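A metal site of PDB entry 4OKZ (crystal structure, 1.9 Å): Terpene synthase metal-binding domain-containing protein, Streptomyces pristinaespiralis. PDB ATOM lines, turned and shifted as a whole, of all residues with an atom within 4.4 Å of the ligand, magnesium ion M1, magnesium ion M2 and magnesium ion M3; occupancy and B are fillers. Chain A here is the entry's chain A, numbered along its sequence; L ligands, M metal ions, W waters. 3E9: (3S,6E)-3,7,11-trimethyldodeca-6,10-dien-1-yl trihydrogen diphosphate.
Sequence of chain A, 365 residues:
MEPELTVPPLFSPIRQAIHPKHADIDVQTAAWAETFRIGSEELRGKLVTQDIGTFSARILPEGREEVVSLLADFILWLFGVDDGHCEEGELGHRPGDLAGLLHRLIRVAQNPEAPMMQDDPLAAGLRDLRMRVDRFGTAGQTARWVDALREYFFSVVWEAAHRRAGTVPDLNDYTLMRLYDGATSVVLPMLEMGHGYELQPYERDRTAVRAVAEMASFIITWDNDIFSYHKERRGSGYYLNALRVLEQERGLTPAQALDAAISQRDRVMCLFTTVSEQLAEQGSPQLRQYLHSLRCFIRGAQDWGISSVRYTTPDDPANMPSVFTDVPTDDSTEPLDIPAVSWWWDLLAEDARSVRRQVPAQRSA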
ATOM      1  N   PHE A  55     -24.085  11.530 -21.798  1.00  0.00           N
ATOM      2  CA  PHE A  55     -24.954  10.544 -21.128  1.00  0.00           C
ATOM      3  C   PHE A  55     -25.987  11.238 -20.241  1.00  0.00           C
ATOM      4  O   PHE A  55     -27.191  10.977 -20.344  1.00  0.00           O
ATOM      5  CB  PHE A  55     -24.064   9.581 -20.325  1.00  0.00           C
ATOM      6  CG  PHE A  55     -24.810   8.546 -19.516  1.00  0.00           C
ATOM      7  CD1 PHE A  55     -26.071   8.077 -19.901  1.00  0.00           C
ATOM      8  CD2 PHE A  55     -24.227   8.010 -18.382  1.00  0.00           C
ATOM      9  CE1 PHE A  55     -26.737   7.123 -19.135  1.00  0.00           C
ATOM     10  CE2 PHE A  55     -24.865   7.050 -17.626  1.00  0.00           C
ATOM     11  CZ  PHE A  55     -26.125   6.603 -18.000  1.00  0.00           C
ATOM     12  N   ILE A  75     -22.017  11.455 -12.007  1.00  0.00           N
ATOM     13  CA  ILE A  75     -21.727  10.190 -12.679  1.00  0.00           C
ATOM     14  C   ILE A  75     -20.203  10.000 -12.824  1.00  0.00           C
ATOM     15  O   ILE A  75     -19.695   8.910 -12.571  1.00  0.00           O
ATOM     16  CB  ILE A  75     -22.423  10.091 -14.058  1.00  0.00           C
ATOM     17  CG1 ILE A  75     -23.940   9.978 -13.850  1.00  0.00           C
ATOM     18  CG2 ILE A  75     -21.933   8.869 -14.830  1.00  0.00           C
ATOM     19  CD1 ILE A  75     -24.762  10.189 -15.102  1.00  0.00           C
ATOM     20  N   LEU A  78     -18.885   9.070  -9.484  1.00  0.00           N
ATOM     21  CA  LEU A  78     -19.226   7.677  -9.182  1.00  0.00           C
ATOM     22  C   LEU A  78     -18.263   6.711  -9.867  1.00  0.00           C
ATOM     23  O   LEU A  78     -17.868   5.720  -9.272  1.00  0.00           O
ATOM     24  CB  LEU A  78     -20.668   7.367  -9.570  1.00  0.00           C
ATOM     25  CG  LEU A  78     -21.762   7.958  -8.663  1.00  0.00           C
ATOM     26  CD1 LEU A  78     -23.125   7.916  -9.347  1.00  0.00           C
ATOM     27  CD2 LEU A  78     -21.806   7.226  -7.334  1.00  0.00           C
ATOM     28  N   PHE A  79     -17.860   7.010 -11.102  1.00  0.00           N
ATOM     29  CA  PHE A  79     -16.825   6.205 -11.771  1.00  0.00           C
ATOM     30  C   PHE A  79     -15.488   6.346 -11.045  1.00  0.00           C
ATOM     31  O   PHE A  79     -14.738   5.378 -10.951  1.00  0.00           O
ATOM     32  CB  PHE A  79     -16.680   6.561 -13.246  1.00  0.00           C
ATOM     33  CG  PHE A  79     -17.732   5.950 -14.115  1.00  0.00           C
ATOM     34  CD1 PHE A  79     -18.636   6.747 -14.814  1.00  0.00           C
ATOM     35  CD2 PHE A  79     -17.845   4.576 -14.228  1.00  0.00           C
ATOM     36  CE1 PHE A  79     -19.609   6.180 -15.607  1.00  0.00           C
ATOM     37  CE2 PHE A  79     -18.817   3.995 -15.021  1.00  0.00           C
ATOM     38  CZ  PHE A  79     -19.702   4.800 -15.712  1.00  0.00           C
ATOM     39  N   ASP A  82     -16.120   3.885  -8.287  1.00  0.00           N
ATOM     40  CA  ASP A  82     -16.365   2.529  -8.749  1.00  0.00           C
ATOM     41  C   ASP A  82     -15.183   1.921  -9.532  1.00  0.00           C
ATOM     42  O   ASP A  82     -14.854   0.752  -9.331  1.00  0.00           O
ATOM     43  CB  ASP A  82     -17.625   2.481  -9.585  1.00  0.00           C
ATOM     44  CG  ASP A  82     -18.285   1.134  -9.539  1.00  0.00           C
ATOM     45  OD1 ASP A  82     -18.714   0.706  -8.454  1.00  0.00           O
ATOM     46  OD2 ASP A  82     -18.368   0.515 -10.606  1.00  0.00           O
ATOM     47  N   ASP A  83     -14.563   2.710 -10.412  1.00  0.00           N
ATOM     48  CA  ASP A  83     -13.331   2.287 -11.078  1.00  0.00           C
ATOM     49  C   ASP A  83     -12.136   2.421 -10.141  1.00  0.00           C
ATOM     50  O   ASP A  83     -11.384   1.466  -9.927  1.00  0.00           O
ATOM     51  CB  ASP A  83     -13.041   3.131 -12.337  1.00  0.00           C
ATOM     52  CG  ASP A  83     -14.023   2.889 -13.465  1.00  0.00           C
ATOM     53  OD1 ASP A  83     -13.975   3.665 -14.445  1.00  0.00           O
ATOM     54  OD2 ASP A  83     -14.814   1.932 -13.404  1.00  0.00           O
ATOM     55  N   GLU A  87     -13.204  -1.445  -8.533  1.00  0.00           N
ATOM     56  CA  GLU A  87     -12.879  -2.406  -9.586  1.00  0.00           C
ATOM     57  C   GLU A  87     -11.424  -2.387 -10.046  1.00  0.00           C
ATOM     58  O   GLU A  87     -10.934  -3.405 -10.550  1.00  0.00           O
ATOM     59  CB  GLU A  87     -13.800  -2.214 -10.782  1.00  0.00           C
ATOM     60  CG  GLU A  87     -15.270  -2.410 -10.467  1.00  0.00           C
ATOM     61  CD  GLU A  87     -16.088  -2.653 -11.710  1.00  0.00           C
ATOM     62  OE1 GLU A  87     -15.980  -3.756 -12.276  1.00  0.00           O
ATOM     63  OE2 GLU A  87     -16.828  -1.742 -12.146  1.00  0.00           O
ATOM     64  N   TYR A 152     -25.933   2.045  -2.624  1.00  0.00           N
ATOM     65  CA  TYR A 152     -24.851   1.764  -3.563  1.00  0.00           C
ATOM     66  C   TYR A 152     -23.580   1.298  -2.833  1.00  0.00           C
ATOM     67  O   TYR A 152     -23.020   0.249  -3.166  1.00  0.00           O
ATOM     68  CB  TYR A 152     -24.564   3.000  -4.438  1.00  0.00           C
ATOM     69  CG  TYR A 152     -23.229   2.965  -5.132  1.00  0.00           C
ATOM     70  CD1 TYR A 152     -22.910   1.941  -6.013  1.00  0.00           C
ATOM     71  CD2 TYR A 152     -22.269   3.940  -4.883  1.00  0.00           C
ATOM     72  CE1 TYR A 152     -21.675   1.882  -6.630  1.00  0.00           C
ATOM     73  CE2 TYR A 152     -21.036   3.895  -5.501  1.00  0.00           C
ATOM     74  CZ  TYR A 152     -20.743   2.862  -6.371  1.00  0.00           C
ATOM     75  OH  TYR A 152     -19.496   2.819  -6.983  1.00  0.00           O
ATOM     76  N   GLU A 159     -20.061  -6.737  -3.238  1.00  0.00           N
ATOM     77  CA  GLU A 159     -19.325  -7.118  -4.452  1.00  0.00           C
ATOM     78  C   GLU A 159     -17.835  -7.346  -4.144  1.00  0.00           C
ATOM     79  O   GLU A 159     -17.218  -8.272  -4.672  1.00  0.00           O
ATOM     80  CB  GLU A 159     -19.485  -6.048  -5.546  1.00  0.00           C
ATOM     81  CG  GLU A 159     -18.856  -6.426  -6.871  1.00  0.00           C
ATOM     82  CD  GLU A 159     -18.791  -5.267  -7.860  1.00  0.00           C
ATOM     83  OE1 GLU A 159     -18.176  -4.232  -7.519  1.00  0.00           O
ATOM     84  OE2 GLU A 159     -19.320  -5.400  -8.972  1.00  0.00           O
ATOM     85  N   ARG A 178     -26.897  -6.246  -7.808  1.00  0.00           N
ATOM     86  CA  ARG A 178     -26.801  -5.434  -9.018  1.00  0.00           C
ATOM     87  C   ARG A 178     -27.873  -4.337  -9.087  1.00  0.00           C
ATOM     88  O   ARG A 178     -27.648  -3.292  -9.703  1.00  0.00           O
ATOM     89  CB  ARG A 178     -26.884  -6.358 -10.244  1.00  0.00           C
ATOM     90  CG  ARG A 178     -26.584  -5.695 -11.583  1.00  0.00           C
ATOM     91  CD  ARG A 178     -25.239  -4.996 -11.590  1.00  0.00           C
ATOM     92  NE  ARG A 178     -24.850  -4.583 -12.941  1.00  0.00           N
ATOM     93  CZ  ARG A 178     -24.029  -3.577 -13.229  1.00  0.00           C
ATOM     94  NH1 ARG A 178     -23.753  -3.295 -14.506  1.00  0.00           N
ATOM     95  NH2 ARG A 178     -23.490  -2.839 -12.263  1.00  0.00           N
ATOM     96  N   ASP A 181     -25.636  -1.865  -7.019  1.00  0.00           N
ATOM     97  CA  ASP A 181     -24.205  -1.617  -7.232  1.00  0.00           C
ATOM     98  C   ASP A 181     -23.891  -0.880  -8.544  1.00  0.00           C
ATOM     99  O   ASP A 181     -22.764  -0.446  -8.748  1.00  0.00           O
ATOM    100  CB  ASP A 181     -23.329  -2.869  -7.015  1.00  0.00           C
ATOM    101  CG  ASP A 181     -23.242  -3.788  -8.224  1.00  0.00           C
ATOM    102  OD1 ASP A 181     -23.088  -5.010  -7.998  1.00  0.00           O
ATOM    103  OD2 ASP A 181     -23.287  -3.317  -9.379  1.00  0.00           O
ATOM    104  N   GLY A 182     -24.904  -0.714  -9.388  1.00  0.00           N
ATOM    105  CA  GLY A 182     -24.808   0.185 -10.545  1.00  0.00           C
ATOM    106  C   GLY A 182     -25.124   1.653 -10.234  1.00  0.00           C
ATOM    107  O   GLY A 182     -25.111   2.486 -11.144  1.00  0.00           O
ATOM    108  N   ALA A 183     -25.429   1.951  -8.967  1.00  0.00           N
ATOM    109  CA  ALA A 183     -25.759   3.310  -8.531  1.00  0.00           C
ATOM    110  C   ALA A 183     -26.966   3.938  -9.225  1.00  0.00           C
ATOM    111  O   ALA A 183     -27.136   5.153  -9.229  1.00  0.00           O
ATOM    112  CB  ALA A 183     -24.532   4.216  -8.646  1.00  0.00           C
ATOM    113  N   THR A 184     -27.829   3.110  -9.805  1.00  0.00           N
ATOM    114  CA  THR A 184     -28.993   3.605 -10.522  1.00  0.00           C
ATOM    115  C   THR A 184     -29.954   4.328  -9.572  1.00  0.00           C
ATOM    116  O   THR A 184     -30.629   5.281  -9.970  1.00  0.00           O
ATOM    117  CB  THR A 184     -29.740   2.468 -11.243  1.00  0.00           C
ATOM    118  OG1 THR A 184     -29.970   1.400 -10.336  1.00  0.00           O
ATOM    119  CG2 THR A 184     -28.913   1.967 -12.428  1.00  0.00           C
ATOM    120  N   VAL A 187     -29.310   8.223  -8.905  1.00  0.00           N
ATOM    121  CA  VAL A 187     -29.694   9.137  -9.983  1.00  0.00           C
ATOM    122  C   VAL A 187     -31.132   9.623  -9.828  1.00  0.00           C
ATOM    123  O   VAL A 187     -31.457  10.757 -10.178  1.00  0.00           O
ATOM    124  CB  VAL A 187     -29.510   8.443 -11.360  1.00  0.00           C
ATOM    125  CG1 VAL A 187     -30.103   9.277 -12.493  1.00  0.00           C
ATOM    126  CG2 VAL A 187     -28.041   8.174 -11.614  1.00  0.00           C
ATOM    127  N   ILE A 220     -31.348  -1.214 -16.936  1.00  0.00           N
ATOM    128  CA  ILE A 220     -30.134  -0.410 -17.109  1.00  0.00           C
ATOM    129  C   ILE A 220     -28.875  -1.236 -16.791  1.00  0.00           C
ATOM    130  O   ILE A 220     -27.909  -1.191 -17.556  1.00  0.00           O
ATOM    131  CB  ILE A 220     -30.198   0.864 -16.244  1.00  0.00           C
ATOM    132  CG1 ILE A 220     -31.241   1.827 -16.830  1.00  0.00           C
ATOM    133  CG2 ILE A 220     -28.835   1.561 -16.167  1.00  0.00           C
ATOM    134  CD1 ILE A 220     -31.666   2.926 -15.876  1.00  0.00           C
ATOM    135  N   THR A 221     -28.900  -1.984 -15.704  1.00  0.00           N
ATOM    136  CA  THR A 221     -27.733  -2.784 -15.318  1.00  0.00           C
ATOM    137  C   THR A 221     -27.543  -4.017 -16.217  1.00  0.00           C
ATOM    138  O   THR A 221     -26.403  -4.380 -16.511  1.00  0.00           O
ATOM    139  CB  THR A 221     -27.766  -3.182 -13.827  1.00  0.00           C
ATOM    140  OG1 THR A 221     -29.002  -3.831 -13.503  1.00  0.00           O
ATOM    141  CG2 THR A 221     -27.590  -1.962 -12.936  1.00  0.00           C
ATOM    142  N   ASN A 224     -26.201  -2.735 -19.437  1.00  0.00           N
ATOM    143  CA  ASN A 224     -24.781  -2.498 -19.221  1.00  0.00           C
ATOM    144  C   ASN A 224     -23.992  -3.798 -19.171  1.00  0.00           C
ATOM    145  O   ASN A 224     -22.938  -3.897 -19.788  1.00  0.00           O
ATOM    146  CB  ASN A 224     -24.536  -1.674 -17.958  1.00  0.00           C
ATOM    147  CG  ASN A 224     -23.064  -1.549 -17.641  1.00  0.00           C
ATOM    148  OD1 ASN A 224     -22.540  -2.332 -16.864  1.00  0.00           O
ATOM    149  ND2 ASN A 224     -22.379  -0.602 -18.268  1.00  0.00           N
ATOM    150  N   SER A 228     -21.166  -3.909 -21.764  1.00  0.00           N
ATOM    151  CA  SER A 228     -19.855  -3.802 -21.114  1.00  0.00           C
ATOM    152  C   SER A 228     -19.148  -5.145 -20.934  1.00  0.00           C
ATOM    153  O   SER A 228     -18.018  -5.191 -20.467  1.00  0.00           O
ATOM    154  CB  SER A 228     -19.949  -3.040 -19.765  1.00  0.00           C
ATOM    155  OG  SER A 228     -20.461  -3.821 -18.687  1.00  0.00           O
ATOM    156  N   LYS A 231     -15.560  -5.169 -22.685  1.00  0.00           N
ATOM    157  CA  LYS A 231     -14.478  -4.464 -21.979  1.00  0.00           C
ATOM    158  C   LYS A 231     -14.172  -5.101 -20.623  1.00  0.00           C
ATOM    159  O   LYS A 231     -13.031  -5.098 -20.173  1.00  0.00           O
ATOM    160  CB  LYS A 231     -14.773  -2.953 -21.856  1.00  0.00           C
ATOM    161  CG  LYS A 231     -15.799  -2.556 -20.797  1.00  0.00           C
ATOM    162  CD  LYS A 231     -15.145  -2.199 -19.462  1.00  0.00           C
ATOM    163  CE  LYS A 231     -16.158  -1.627 -18.488  1.00  0.00           C
ATOM    164  NZ  LYS A 231     -15.559  -1.345 -17.153  1.00  0.00           N
ATOM    165  N   GLU A 232     -15.195  -5.665 -19.982  1.00  0.00           N
ATOM    166  CA  GLU A 232     -15.028  -6.299 -18.664  1.00  0.00           C
ATOM    167  C   GLU A 232     -14.281  -7.621 -18.729  1.00  0.00           C
ATOM    168  O   GLU A 232     -13.327  -7.830 -17.975  1.00  0.00           O
ATOM    169  CB  GLU A 232     -16.377  -6.486 -17.983  1.00  0.00           C
ATOM    170  CG  GLU A 232     -16.912  -5.172 -17.469  1.00  0.00           C
ATOM    171  CD  GLU A 232     -18.308  -5.245 -16.864  1.00  0.00           C
ATOM    172  OE1 GLU A 232     -18.704  -4.205 -16.331  1.00  0.00           O
ATOM    173  OE2 GLU A 232     -18.989  -6.292 -16.918  1.00  0.00           O
ATOM    174  N   PHE A 297     -33.914   7.745 -18.738  1.00  0.00           N
ATOM    175  CA  PHE A 297     -32.749   7.141 -18.095  1.00  0.00           C
ATOM    176  C   PHE A 297     -32.421   5.807 -18.771  1.00  0.00           C
ATOM    177  O   PHE A 297     -31.284   5.547 -19.133  1.00  0.00           O
ATOM    178  CB  PHE A 297     -33.053   6.981 -16.592  1.00  0.00           C
ATOM    179  CG  PHE A 297     -31.879   6.550 -15.731  1.00  0.00           C
ATOM    180  CD1 PHE A 297     -30.555   6.603 -16.181  1.00  0.00           C
ATOM    181  CD2 PHE A 297     -32.112   6.145 -14.422  1.00  0.00           C
ATOM    182  CE1 PHE A 297     -29.509   6.219 -15.353  1.00  0.00           C
ATOM    183  CE2 PHE A 297     -31.066   5.760 -13.594  1.00  0.00           C
ATOM    184  CZ  PHE A 297     -29.761   5.805 -14.052  1.00  0.00           C
ATOM    185  N   TRP A 304     -25.948   5.574 -24.934  1.00  0.00           N
ATOM    186  CA  TRP A 304     -24.590   5.799 -24.439  1.00  0.00           C
ATOM    187  C   TRP A 304     -23.793   4.498 -24.408  1.00  0.00           C
ATOM    188  O   TRP A 304     -22.613   4.476 -24.755  1.00  0.00           O
ATOM    189  CB  TRP A 304     -24.661   6.437 -23.046  1.00  0.00           C
ATOM    190  CG  TRP A 304     -23.339   6.783 -22.471  1.00  0.00           C
ATOM    191  CD1 TRP A 304     -22.443   7.687 -22.953  1.00  0.00           C
ATOM    192  CD2 TRP A 304     -22.780   6.248 -21.282  1.00  0.00           C
ATOM    193  NE1 TRP A 304     -21.346   7.738 -22.132  1.00  0.00           N
ATOM    194  CE2 TRP A 304     -21.524   6.863 -21.097  1.00  0.00           C
ATOM    195  CE3 TRP A 304     -23.215   5.303 -20.332  1.00  0.00           C
ATOM    196  CZ2 TRP A 304     -20.699   6.561 -20.016  1.00  0.00           C
ATOM    197  CZ3 TRP A 304     -22.394   5.006 -19.264  1.00  0.00           C
ATOM    198  CH2 TRP A 304     -21.148   5.641 -19.116  1.00  0.00           C
ATOM    199  N   ARG A 310     -15.788   3.989 -23.632  1.00  0.00           N
ATOM    200  CA  ARG A 310     -15.748   3.113 -22.472  1.00  0.00           C
ATOM    201  C   ARG A 310     -16.140   1.673 -22.843  1.00  0.00           C
ATOM    202  O   ARG A 310     -15.590   0.711 -22.313  1.00  0.00           O
ATOM    203  CB  ARG A 310     -16.683   3.666 -21.388  1.00  0.00           C
ATOM    204  CG  ARG A 310     -16.418   3.084 -20.019  1.00  0.00           C
ATOM    205  CD  ARG A 310     -17.373   3.627 -18.976  1.00  0.00           C
ATOM    206  NE  ARG A 310     -17.209   2.832 -17.765  1.00  0.00           N
ATOM    207  CZ  ARG A 310     -16.232   3.007 -16.866  1.00  0.00           C
ATOM    208  NH1 ARG A 310     -16.170   2.191 -15.828  1.00  0.00           N
ATOM    209  NH2 ARG A 310     -15.338   3.982 -16.992  1.00  0.00           N
ATOM    210  N   TYR A 311     -17.105   1.534 -23.759  1.00  0.00           N
ATOM    211  CA  TYR A 311     -17.635   0.220 -24.136  1.00  0.00           C
ATOM    212  C   TYR A 311     -17.208  -0.238 -25.534  1.00  0.00           C
ATOM    213  O   TYR A 311     -17.000  -1.426 -25.753  1.00  0.00           O
ATOM    214  CB  TYR A 311     -19.153   0.239 -24.008  1.00  0.00           C
ATOM    215  CG  TYR A 311     -19.605   0.744 -22.654  1.00  0.00           C
ATOM    216  CD1 TYR A 311     -20.313   1.937 -22.527  1.00  0.00           C
ATOM    217  CD2 TYR A 311     -19.267   0.051 -21.490  1.00  0.00           C
ATOM    218  CE1 TYR A 311     -20.699   2.413 -21.286  1.00  0.00           C
ATOM    219  CE2 TYR A 311     -19.657   0.527 -20.240  1.00  0.00           C
ATOM    220  CZ  TYR A 311     -20.366   1.704 -20.146  1.00  0.00           C
ATOM    221  OH  TYR A 311     -20.751   2.166 -18.904  1.00  0.00           O
HETATM  222  C1  3E9 L   1     -22.134   0.807 -13.159  1.00  0.00           C
HETATM  223  O1  3E9 L   1     -21.772  -0.558 -13.289  1.00  0.00           O
HETATM  224  C2  3E9 L   1     -21.333   1.351 -11.993  1.00  0.00           C
HETATM  225  C3  3E9 L   1     -21.786   2.804 -11.664  1.00  0.00           C
HETATM  226  C4  3E9 L   1     -21.420   3.097 -10.200  1.00  0.00           C
HETATM  227  C5  3E9 L   1     -21.158   3.818 -12.609  1.00  0.00           C
HETATM  228  C6  3E9 L   1     -21.936   5.111 -12.372  1.00  0.00           C
HETATM  229  C7  3E9 L   1     -23.060   5.168 -13.424  1.00  0.00           C
HETATM  230  C8  3E9 L   1     -24.476   5.651 -13.064  1.00  0.00           C
HETATM  231  C10 3E9 L   1     -24.858   6.182 -11.681  1.00  0.00           C
HETATM  232  C9  3E9 L   1     -25.532   5.641 -14.118  1.00  0.00           C
HETATM  233  C11 3E9 L   1     -25.894   4.178 -14.281  1.00  0.00           C
HETATM  234  C12 3E9 L   1     -25.265   3.729 -15.593  1.00  0.00           C
HETATM  235  C13 3E9 L   1     -24.941   2.256 -15.867  1.00  0.00           C
HETATM  236  C14 3E9 L   1     -24.349   1.903 -17.218  1.00  0.00           C
HETATM  237  C15 3E9 L   1     -25.184   1.135 -14.845  1.00  0.00           C
HETATM  238  PA  3E9 L   1     -20.409  -1.101 -13.985  1.00  0.00           P
HETATM  239  O1A 3E9 L   1     -20.783  -2.444 -14.784  1.00  0.00           O
HETATM  240  O2A 3E9 L   1     -19.507  -1.479 -12.946  1.00  0.00           O
HETATM  241  O3A 3E9 L   1     -19.980   0.055 -14.962  1.00  0.00           O
HETATM  242  PB  3E9 L   1     -18.901  -0.205 -16.044  1.00  0.00           P
HETATM  243  O1B 3E9 L   1     -19.609  -1.313 -16.955  1.00  0.00           O
HETATM  244  O2B 3E9 L   1     -19.123   0.954 -16.937  1.00  0.00           O
HETATM  245  O3B 3E9 L   1     -17.560  -0.545 -15.634  1.00  0.00           O
HETATM  246 MG    MG M   1     -20.549  -3.145 -16.715  1.00  0.00          MG
HETATM  247 MG    MG M   2     -17.610  -1.018 -13.704  1.00  0.00          MG
HETATM  248 MG    MG M   3     -18.933  -1.525 -10.976  1.00  0.00          MG
HETATM  249  O   HOH W   1     -21.365  -4.929 -16.229  1.00  0.00           O
HETATM  250  O   HOH W   2     -20.905  -1.424 -10.389  1.00  0.00           O
HETATM  251  O   HOH W   3     -15.243  -0.683 -14.164  1.00  0.00           O
HETATM  252  O   HOH W   4     -19.851  -4.914 -13.450  1.00  0.00           O
HETATM  253  O   HOH W   5     -23.579   1.255 -19.901  1.00  0.00           O
HETATM  254  O   HOH W   6     -17.129  -2.947 -14.588  1.00  0.00           O
HETATM  255  O   HOH W   7     -18.281  -2.033  -8.988  1.00  0.00           O
HETATM  256  O   HOH W   8     -17.292   0.975 -13.069  1.00  0.00           O
HETATM  257  O   HOH W   9     -19.273  -3.541 -11.153  1.00  0.00           O
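Two residues have an atom within 4 Å of magnesium ion M3: Asp 82 and Glu 87.
Arg 178 touches magnesium ion M1 (NH1 to MG, 3.9 Å). The nearest printed residue that does not touch magnesium ion M1 is Lys 231 (5.0 Å).
NZ of Lys 231 lies close to O3B of the ligand (2.6 Å). An oxygen (O2B) of the ligand is in salt-bridge range of the guanidinium group (NE) of Arg 310 (2.8 Å). The side-chain hydroxyl (OH) of Tyr 311 sits at hydrogen-bond distance from an oxygen (O2B) of the ligand, 2.8 Å away. The guanidinium group (NH2) of Arg 178 lies within hydrogen-bond range of an oxygen (O1) of the ligand (3.0 Å).
Magnesium ion M3 is bound by water W9 (2.1 Å), an oxygen (O2A) of the ligand (2.1 Å), water W2 (2.1 Å), the side-chain carboxylate (OD2) of Asp 82 (2.1 Å), water W7 (2.2 Å) and the side-chain carboxylate (OE2) of Glu 87 (2.4 Å).
Phe 55 touches the ligand. Leu 78 touches the ligand. Phe 79 touches the ligand (CE2 to C5, 3.4 Å). OH of Tyr 152 touches C4 of the ligand, at 3.8 Å. Asp 181 touches the ligand. Gly 182 touches the ligand (O to C3, 3.4 Å). O of Ala 183 touches C10 of the ligand, 3.5 Å away. Val 187 touches the ligand (CG2 to C10, 3.8 Å). CG2 of Ile 220 touches C15 of the ligand, 3.9 Å away. Hydrophobic or aromatic side chains that line the ligand: Phe 55, Leu 78, Phe 79, Tyr 152, Ala 183, Val 187, Ile 220 and Tyr 311. The nearest printed residue that does not touch the ligand is Ile 75 (4.1 Å).
Magnesium ion M2 is bound by the side-chain carboxylate of Glu 87 (1.9 Å), an oxygen (O3B) of the ligand (2.0 Å), an oxygen (O2A) of the ligand (2.1 Å), water W8 (2.1 Å), water W6 (2.2 Å) and water W3 (2.4 Å). Magnesium ion M2 has six donor atoms within binding distance.
Of the 25 residues printed, 2 come within 4 Å of magnesium ion M2.
ND2 of Asn 224 is in hydrogen-bond range of OH of Tyr 311, at 3.3 Å. The guanidinium group (NH1) of Arg 178 sits close to the side-chain amide oxygen (OD1) of Asn 224 (2.8 Å). The guanidinium group (NH1) of Arg 310 lies within salt-bridge range of the side-chain carboxylate (OD2) of Asp 83 (2.8 Å). The side-chain carboxylate of Asp 181 is in salt-bridge range of the guanidinium group of Arg 178, 2.9 Å away. O of Thr 221 sits at hydrogen-bond distance from NH1 of Arg 178, at 3.5 Å. OD1 of Asp 82 sits at hydrogen-bond distance from OH of Tyr 152, 2.7 Å away.
Magnesium ion M1 is bound by water W1 (2.0 Å). O1A of the ligand is bound to magnesium ion M1 (2.1 Å). Magnesium ion M1 is bound by an oxygen (O1B) of the ligand (2.1 Å). Magnesium ion M1 is bound by the side-chain hydroxyl (OG) of Ser 228, at 2.1 Å. Magnesium ion M1 is bound by OD1 of Asn 224. OE1 of Glu 232 is bound to magnesium ion M1, at 2.2 Å. Magnesium ion M1 has six donor atoms within binding distance.
Water W8 lies within hydrogen-bond range of OD2 of Asp 83, NH1 of Arg 310 and O3A of the ligand. Water W3 lies within hydrogen-bond range of the side-chain carboxylate of Asp 83, the side-chain amino group of Lys 231 and the guanidinium group of Arg 310. Water W6 bridges the side-chain carboxylate (OE1) of Glu 87 (2.7 Å) and the side-chain amino group (NZ) of Lys 231 (3.4 Å). Water W7 lies within hydrogen-bond range of OE1 of Glu 159 (2.6 Å) and OD1 of Asp 82 (2.8 Å). Water W2 lies within hydrogen-bond range of the backbone carbonyl oxygen of Asp 181 (2.7 Å), an oxygen (O1) of the ligand (3.1 Å) and the guanidinium group of Arg 178 (3.5 Å). Water W5 bridges ND2 of Asn 224 and OH of Tyr 311.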
